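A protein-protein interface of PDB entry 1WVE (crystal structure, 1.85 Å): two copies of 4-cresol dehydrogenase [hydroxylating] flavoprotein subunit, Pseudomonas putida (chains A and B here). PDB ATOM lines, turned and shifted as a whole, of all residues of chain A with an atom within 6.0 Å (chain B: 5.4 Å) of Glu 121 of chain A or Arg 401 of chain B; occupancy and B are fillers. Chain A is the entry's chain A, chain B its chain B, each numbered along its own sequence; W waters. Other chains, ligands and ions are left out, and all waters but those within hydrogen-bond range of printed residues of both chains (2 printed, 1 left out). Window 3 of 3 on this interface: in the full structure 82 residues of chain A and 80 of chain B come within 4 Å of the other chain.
The side-chain carboxylate (OD2) of Asp 119 of chain A lies within salt-bridge range of the guanidinium group (NH2) of Arg 401 of chain B (3.6 Å). The side-chain carboxylate of Glu 121 of chain A is in salt-bridge range of the guanidinium group of Arg 401 of chain B (3.4 Å).
The backbone NH (N) of Met 122 of chain A lies within hydrogen-bond range of the side-chain carboxylate (OD1) of Asp 119 of chain A (2.8 Å). The backbone NH (N) of Asp 119 of chain A is in hydrogen-bond range of the backbone carbonyl oxygen (O) of Tyr 124 of chain A, 2.9 Å away. The guanidinium group (NH1) of Arg 265 of chain B lies within salt-bridge range of the side-chain carboxylate (OD1) of Asp 262 of chain B (3.0 Å). The guanidinium group (NH1) of Arg 265 of chain B is in hydrogen-bond range of the backbone carbonyl oxygen (O) of Ala 400 of chain B (3.1 Å). The side-chain carboxylate of Glu 399 of chain B lies within salt-bridge range of the guanidinium group of Arg 401 of chain B. SG of Cys 405 of chain B is in hydrogen-bond range of O of Glu 399 of chain B (3.7 Å).
Arg 265 of chain B touches Glu 121 of chain A. Met 269 of chain B touches Glu 121 of chain A (CE to O, 3.5 Å). Met 122 of chain A touches Arg 265 of chain B. CE of Met 269 of chain B touches O of Met 122 of chain A, 3.7 Å away. Glu 399 of chain B touches Met 122 of chain A. Met 122 of chain A touches Ala 400 of chain B (CE to N, 3.7 Å). Arg 401 of chain B touches Met 122 of chain A (NH2 to CG, 3.2 Å).
Printed residues of chain B within 4 Å of Asp 119 of chain A: Arg 401 (3.6 Å). Of the printed residues of chain B, Glu 121 of chain A touches Arg 265, Met 269 and Arg 401. Of the printed residues of chain B, Met 122 of chain A touches Arg 265, Met 269, Glu 399, Ala 400 and Arg 401. Cys 123 of chain A touches none of the printed residues of chain B. Printed residues of chain A within 4 Å of Arg 265 of chain B: Glu 121 (3.8 Å) and Met 122 (3.8 Å). Of the printed residues of chain A, Met 269 of chain B touches Glu 121 and Met 122. Of the printed residues of chain A, Ala 400 of chain B touches Met 122. Of the printed residues of chain A, Arg 401 of chain B touches Asp 119 (3.6 Å), Glu 121 (3.4 Å) and Met 122 (3.2 Å). Lys 406 of chain B touches none of the printed residues of chain A.
Of the 14 printed residues of chain B, 5 touch a printed residue of chain A. Hydrophobic or aromatic side chains of chain B within 4 Å of the printed part of chain A: Met 269. Among the printed residues, 9 pairs touch across the chains. Among the printed residues, Asp or Glu carboxylates within 4 Å of a Lys or Arg side-chain nitrogen of the other chain: Asp 119 of chain A with Arg 401 of chain B and Glu 121 of chain A with Arg 401 of chain B.
No position is printed for both chains.
Water W2 lies within hydrogen-bond range of OE1 of Glu 399 of chain B (2.5 Å) and OH of Tyr 124 of chain A (2.8 Å). Water W1 bridges the backbone carbonyl oxygen (O) of Glu 121 of chain A (2.7 Å) and the guanidinium group (NE) of Arg 265 of chain B (3.0 Å).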
ATOM      1  N   ASP A 119     -26.583   0.437  23.528  1.00  0.00           N
ATOM      2  CA  ASP A 119     -25.976   1.726  23.216  1.00  0.00           C
ATOM      3  C   ASP A 119     -27.115   2.649  22.782  1.00  0.00           C
ATOM      4  O   ASP A 119     -27.726   2.431  21.735  1.00  0.00           O
ATOM      5  CB  ASP A 119     -24.960   1.543  22.078  1.00  0.00           C
ATOM      6  CG  ASP A 119     -24.178   2.814  21.764  1.00  0.00           C
ATOM      7  OD1 ASP A 119     -24.768   3.919  21.759  1.00  0.00           O
ATOM      8  OD2 ASP A 119     -22.970   2.704  21.495  1.00  0.00           O
ATOM      9  N   PRO A 120     -27.428   3.683  23.588  1.00  0.00           N
ATOM     10  CA  PRO A 120     -28.510   4.615  23.251  1.00  0.00           C
ATOM     11  C   PRO A 120     -28.194   5.643  22.162  1.00  0.00           C
ATOM     12  O   PRO A 120     -29.095   6.322  21.682  1.00  0.00           O
ATOM     13  CB  PRO A 120     -28.820   5.279  24.599  1.00  0.00           C
ATOM     14  CG  PRO A 120     -27.466   5.381  25.213  1.00  0.00           C
ATOM     15  CD  PRO A 120     -26.874   3.993  24.920  1.00  0.00           C
ATOM     16  N   GLU A 121     -26.927   5.758  21.774  1.00  0.00           N
ATOM     17  CA  GLU A 121     -26.521   6.717  20.744  1.00  0.00           C
ATOM     18  C   GLU A 121     -26.419   6.051  19.377  1.00  0.00           C
ATOM     19  O   GLU A 121     -26.932   6.568  18.388  1.00  0.00           O
ATOM     20  CB  GLU A 121     -25.171   7.343  21.101  1.00  0.00           C
ATOM     21  CG  GLU A 121     -25.195   8.229  22.341  1.00  0.00           C
ATOM     22  CD  GLU A 121     -23.795   8.601  22.815  1.00  0.00           C
ATOM     23  OE1 GLU A 121     -23.008   9.136  21.997  1.00  0.00           O
ATOM     24  OE2 GLU A 121     -23.485   8.355  24.006  1.00  0.00           O
ATOM     25  N   MET A 122     -25.731   4.914  19.321  1.00  0.00           N
ATOM     26  CA  MET A 122     -25.599   4.175  18.065  1.00  0.00           C
ATOM     27  C   MET A 122     -26.842   3.298  17.903  1.00  0.00           C
ATOM     28  O   MET A 122     -27.036   2.644  16.878  1.00  0.00           O
ATOM     29  CB  MET A 122     -24.328   3.316  18.065  1.00  0.00           C
ATOM     30  CG  MET A 122     -23.025   4.103  18.176  1.00  0.00           C
ATOM     31  SD  MET A 122     -22.974   5.593  17.121  1.00  0.00           S
ATOM     32  CE  MET A 122     -23.116   4.861  15.500  1.00  0.00           C
ATOM     33  N   CYS A 123     -27.670   3.290  18.942  1.00  0.00           N
ATOM     34  CA  CYS A 123     -28.916   2.544  18.962  1.00  0.00           C
ATOM     35  C   CYS A 123     -28.848   1.070  18.577  1.00  0.00           C
ATOM     36  O   CYS A 123     -29.301   0.665  17.500  1.00  0.00           O
ATOM     37  CB  CYS A 123     -29.949   3.263  18.092  1.00  0.00           C
ATOM     38  SG  CYS A 123     -30.406   4.904  18.759  1.00  0.00           S
ATOM     39  N   TYR A 124     -28.280   0.270  19.468  1.00  0.00           N
ATOM     40  CA  TYR A 124     -28.213  -1.166  19.245  1.00  0.00           C
ATOM     41  C   TYR A 124     -28.136  -1.879  20.580  1.00  0.00           C
ATOM     42  O   TYR A 124     -27.915  -1.263  21.620  1.00  0.00           O
ATOM     43  CB  TYR A 124     -27.003  -1.554  18.383  1.00  0.00           C
ATOM     44  CG  TYR A 124     -25.651  -1.333  19.026  1.00  0.00           C
ATOM     45  CD1 TYR A 124     -25.178  -2.187  20.027  1.00  0.00           C
ATOM     46  CD2 TYR A 124     -24.811  -0.317  18.580  1.00  0.00           C
ATOM     47  CE1 TYR A 124     -23.895  -2.033  20.549  1.00  0.00           C
ATOM     48  CE2 TYR A 124     -23.527  -0.152  19.100  1.00  0.00           C
ATOM     49  CZ  TYR A 124     -23.075  -1.016  20.078  1.00  0.00           C
ATOM     50  OH  TYR A 124     -21.800  -0.878  20.569  1.00  0.00           O
ATOM     51  N   VAL B 261     -20.517  14.728  11.539  1.00  0.00           N
ATOM     52  CA  VAL B 261     -21.013  13.368  11.707  1.00  0.00           C
ATOM     53  C   VAL B 261     -22.010  13.224  12.862  1.00  0.00           C
ATOM     54  O   VAL B 261     -23.054  12.563  12.721  1.00  0.00           O
ATOM     55  CB  VAL B 261     -19.830  12.393  11.884  1.00  0.00           C
ATOM     56  CG1 VAL B 261     -20.325  10.985  12.198  1.00  0.00           C
ATOM     57  CG2 VAL B 261     -19.003  12.376  10.595  1.00  0.00           C
ATOM     58  N   ASP B 262     -21.720  13.859  13.993  1.00  0.00           N
ATOM     59  CA  ASP B 262     -22.615  13.733  15.137  1.00  0.00           C
ATOM     60  C   ASP B 262     -23.960  14.405  14.907  1.00  0.00           C
ATOM     61  O   ASP B 262     -24.968  13.975  15.456  1.00  0.00           O
ATOM     62  CB  ASP B 262     -21.941  14.264  16.410  1.00  0.00           C
ATOM     63  CG  ASP B 262     -20.756  13.408  16.835  1.00  0.00           C
ATOM     64  OD1 ASP B 262     -20.739  12.203  16.498  1.00  0.00           O
ATOM     65  OD2 ASP B 262     -19.851  13.923  17.516  1.00  0.00           O
ATOM     66  N   ARG B 265     -25.793  11.933  12.113  1.00  0.00           N
ATOM     67  CA  ARG B 265     -26.256  10.632  12.591  1.00  0.00           C
ATOM     68  C   ARG B 265     -27.751  10.558  12.935  1.00  0.00           C
ATOM     69  O   ARG B 265     -28.461   9.692  12.426  1.00  0.00           O
ATOM     70  CB  ARG B 265     -25.398  10.163  13.781  1.00  0.00           C
ATOM     71  CG  ARG B 265     -25.839   8.812  14.377  1.00  0.00           C
ATOM     72  CD  ARG B 265     -24.943   8.369  15.544  1.00  0.00           C
ATOM     73  NE  ARG B 265     -24.987   9.303  16.664  1.00  0.00           N
ATOM     74  CZ  ARG B 265     -24.004  10.135  16.992  1.00  0.00           C
ATOM     75  NH1 ARG B 265     -22.880  10.151  16.292  1.00  0.00           N
ATOM     76  NH2 ARG B 265     -24.152  10.970  18.014  1.00  0.00           N
ATOM     77  N   MET B 269     -30.393   8.191  11.175  1.00  0.00           N
ATOM     78  CA  MET B 269     -31.025   7.221  12.068  1.00  0.00           C
ATOM     79  C   MET B 269     -32.559   7.297  12.045  1.00  0.00           C
ATOM     80  O   MET B 269     -33.241   6.274  12.158  1.00  0.00           O
ATOM     81  CB  MET B 269     -30.518   7.446  13.495  1.00  0.00           C
ATOM     82  CG  MET B 269     -30.588   6.230  14.419  1.00  0.00           C
ATOM     83  SD  MET B 269     -29.261   5.035  14.138  1.00  0.00           S
ATOM     84  CE  MET B 269     -27.950   5.769  15.123  1.00  0.00           C
ATOM     85  N   SER B 398     -16.246   2.128  10.019  1.00  0.00           N
ATOM     86  CA  SER B 398     -16.214   2.911  11.244  1.00  0.00           C
ATOM     87  C   SER B 398     -17.598   3.170  11.811  1.00  0.00           C
ATOM     88  O   SER B 398     -18.596   3.112  11.094  1.00  0.00           O
ATOM     89  CB  SER B 398     -15.524   4.254  10.967  1.00  0.00           C
ATOM     90  OG  SER B 398     -15.698   5.171  12.042  1.00  0.00           O
ATOM     91  N   GLU B 399     -17.659   3.429  13.111  1.00  0.00           N
ATOM     92  CA  GLU B 399     -18.911   3.819  13.741  1.00  0.00           C
ATOM     93  C   GLU B 399     -19.201   5.193  13.119  1.00  0.00           C
ATOM     94  O   GLU B 399     -18.265   5.943  12.822  1.00  0.00           O
ATOM     95  CB  GLU B 399     -18.724   4.079  15.232  1.00  0.00           C
ATOM     96  CG  GLU B 399     -19.007   2.934  16.167  1.00  0.00           C
ATOM     97  CD  GLU B 399     -18.973   3.387  17.614  1.00  0.00           C
ATOM     98  OE1 GLU B 399     -19.621   2.732  18.455  1.00  0.00           O
ATOM     99  OE2 GLU B 399     -18.294   4.399  17.903  1.00  0.00           O
ATOM    100  N   ALA B 400     -20.472   5.532  12.934  1.00  0.00           N
ATOM    101  CA  ALA B 400     -20.827   6.846  12.414  1.00  0.00           C
ATOM    102  C   ALA B 400     -20.810   7.770  13.634  1.00  0.00           C
ATOM    103  O   ALA B 400     -21.844   8.307  14.059  1.00  0.00           O
ATOM    104  CB  ALA B 400     -22.205   6.815  11.784  1.00  0.00           C
ATOM    105  N   ARG B 401     -19.619   7.940  14.202  1.00  0.00           N
ATOM    106  CA  ARG B 401     -19.420   8.772  15.381  1.00  0.00           C
ATOM    107  C   ARG B 401     -18.289   9.755  15.063  1.00  0.00           C
ATOM    108  O   ARG B 401     -17.208   9.350  14.635  1.00  0.00           O
ATOM    109  CB  ARG B 401     -19.046   7.880  16.575  1.00  0.00           C
ATOM    110  CG  ARG B 401     -19.276   8.500  17.947  1.00  0.00           C
ATOM    111  CD  ARG B 401     -18.522   7.740  19.038  1.00  0.00           C
ATOM    112  NE  ARG B 401     -19.012   6.379  19.241  1.00  0.00           N
ATOM    113  CZ  ARG B 401     -20.112   6.072  19.922  1.00  0.00           C
ATOM    114  NH1 ARG B 401     -20.843   7.032  20.471  1.00  0.00           N
ATOM    115  NH2 ARG B 401     -20.483   4.805  20.058  1.00  0.00           N
ATOM    116  N   GLY B 402     -18.550  11.044  15.265  1.00  0.00           N
ATOM    117  CA  GLY B 402     -17.562  12.073  14.981  1.00  0.00           C
ATOM    118  C   GLY B 402     -16.122  11.833  15.410  1.00  0.00           C
ATOM    119  O   GLY B 402     -15.198  12.022  14.619  1.00  0.00           O
ATOM    120  N   SER B 403     -15.917  11.426  16.659  1.00  0.00           N
ATOM    121  CA  SER B 403     -14.571  11.179  17.153  1.00  0.00           C
ATOM    122  C   SER B 403     -13.873  10.035  16.401  1.00  0.00           C
ATOM    123  O   SER B 403     -12.670  10.103  16.131  1.00  0.00           O
ATOM    124  CB  SER B 403     -14.616  10.858  18.650  1.00  0.00           C
ATOM    125  OG  SER B 403     -15.441   9.734  18.905  1.00  0.00           O
ATOM    126  N   GLU B 404     -14.623   8.982  16.079  1.00  0.00           N
ATOM    127  CA  GLU B 404     -14.057   7.839  15.366  1.00  0.00           C
ATOM    128  C   GLU B 404     -13.604   8.258  13.984  1.00  0.00           C
ATOM    129  O   GLU B 404     -12.485   7.959  13.562  1.00  0.00           O
ATOM    130  CB  GLU B 404     -15.083   6.708  15.224  1.00  0.00           C
ATOM    131  CG  GLU B 404     -15.267   5.846  16.461  1.00  0.00           C
ATOM    132  CD  GLU B 404     -13.986   5.183  16.902  1.00  0.00           C
ATOM    133  OE1 GLU B 404     -13.335   5.686  17.842  1.00  0.00           O
ATOM    134  OE2 GLU B 404     -13.615   4.154  16.306  1.00  0.00           O
ATOM    135  N   CYS B 405     -14.484   8.953  13.280  1.00  0.00           N
ATOM    136  CA  CYS B 405     -14.171   9.405  11.937  1.00  0.00           C
ATOM    137  C   CYS B 405     -12.960  10.339  11.927  1.00  0.00           C
ATOM    138  O   CYS B 405     -12.133  10.264  11.025  1.00  0.00           O
ATOM    139  CB  CYS B 405     -15.408  10.070  11.306  1.00  0.00           C
ATOM    140  SG  CYS B 405     -16.798   8.904  11.050  1.00  0.00           S
ATOM    141  N   LYS B 406     -12.841  11.201  12.932  1.00  0.00           N
ATOM    142  CA  LYS B 406     -11.696  12.114  13.009  1.00  0.00           C
ATOM    143  C   LYS B 406     -10.397  11.333  13.280  1.00  0.00           C
ATOM    144  O   LYS B 406      -9.344  11.624  12.710  1.00  0.00           O
ATOM    145  CB  LYS B 406     -11.910  13.134  14.125  1.00  0.00           C
ATOM    146  CG  LYS B 406     -10.697  14.011  14.395  1.00  0.00           C
ATOM    147  CD  LYS B 406     -10.892  14.829  15.647  1.00  0.00           C
ATOM    148  CE  LYS B 406      -9.597  15.490  16.077  1.00  0.00           C
ATOM    149  NZ  LYS B 406      -9.776  16.215  17.362  1.00  0.00           N
ATOM    150  N   MET B 434     -19.985   3.788   8.780  1.00  0.00           N
ATOM    151  CA  MET B 434     -19.316   4.593   7.760  1.00  0.00           C
ATOM    152  C   MET B 434     -18.447   3.688   6.904  1.00  0.00           C
ATOM    153  O   MET B 434     -17.724   2.842   7.441  1.00  0.00           O
ATOM    154  CB  MET B 434     -18.366   5.612   8.386  1.00  0.00           C
ATOM    155  CG  MET B 434     -19.024   6.605   9.287  1.00  0.00           C
ATOM    156  SD  MET B 434     -20.207   7.546   8.337  1.00  0.00           S
ATOM    157  CE  MET B 434     -20.029   9.182   9.139  1.00  0.00           C
HETATM  158  O   HOH W   1     -27.845   9.019  17.556  1.00  0.00           O
HETATM  159  O   HOH W   2     -19.818   0.356  19.029  1.00  0.00           O
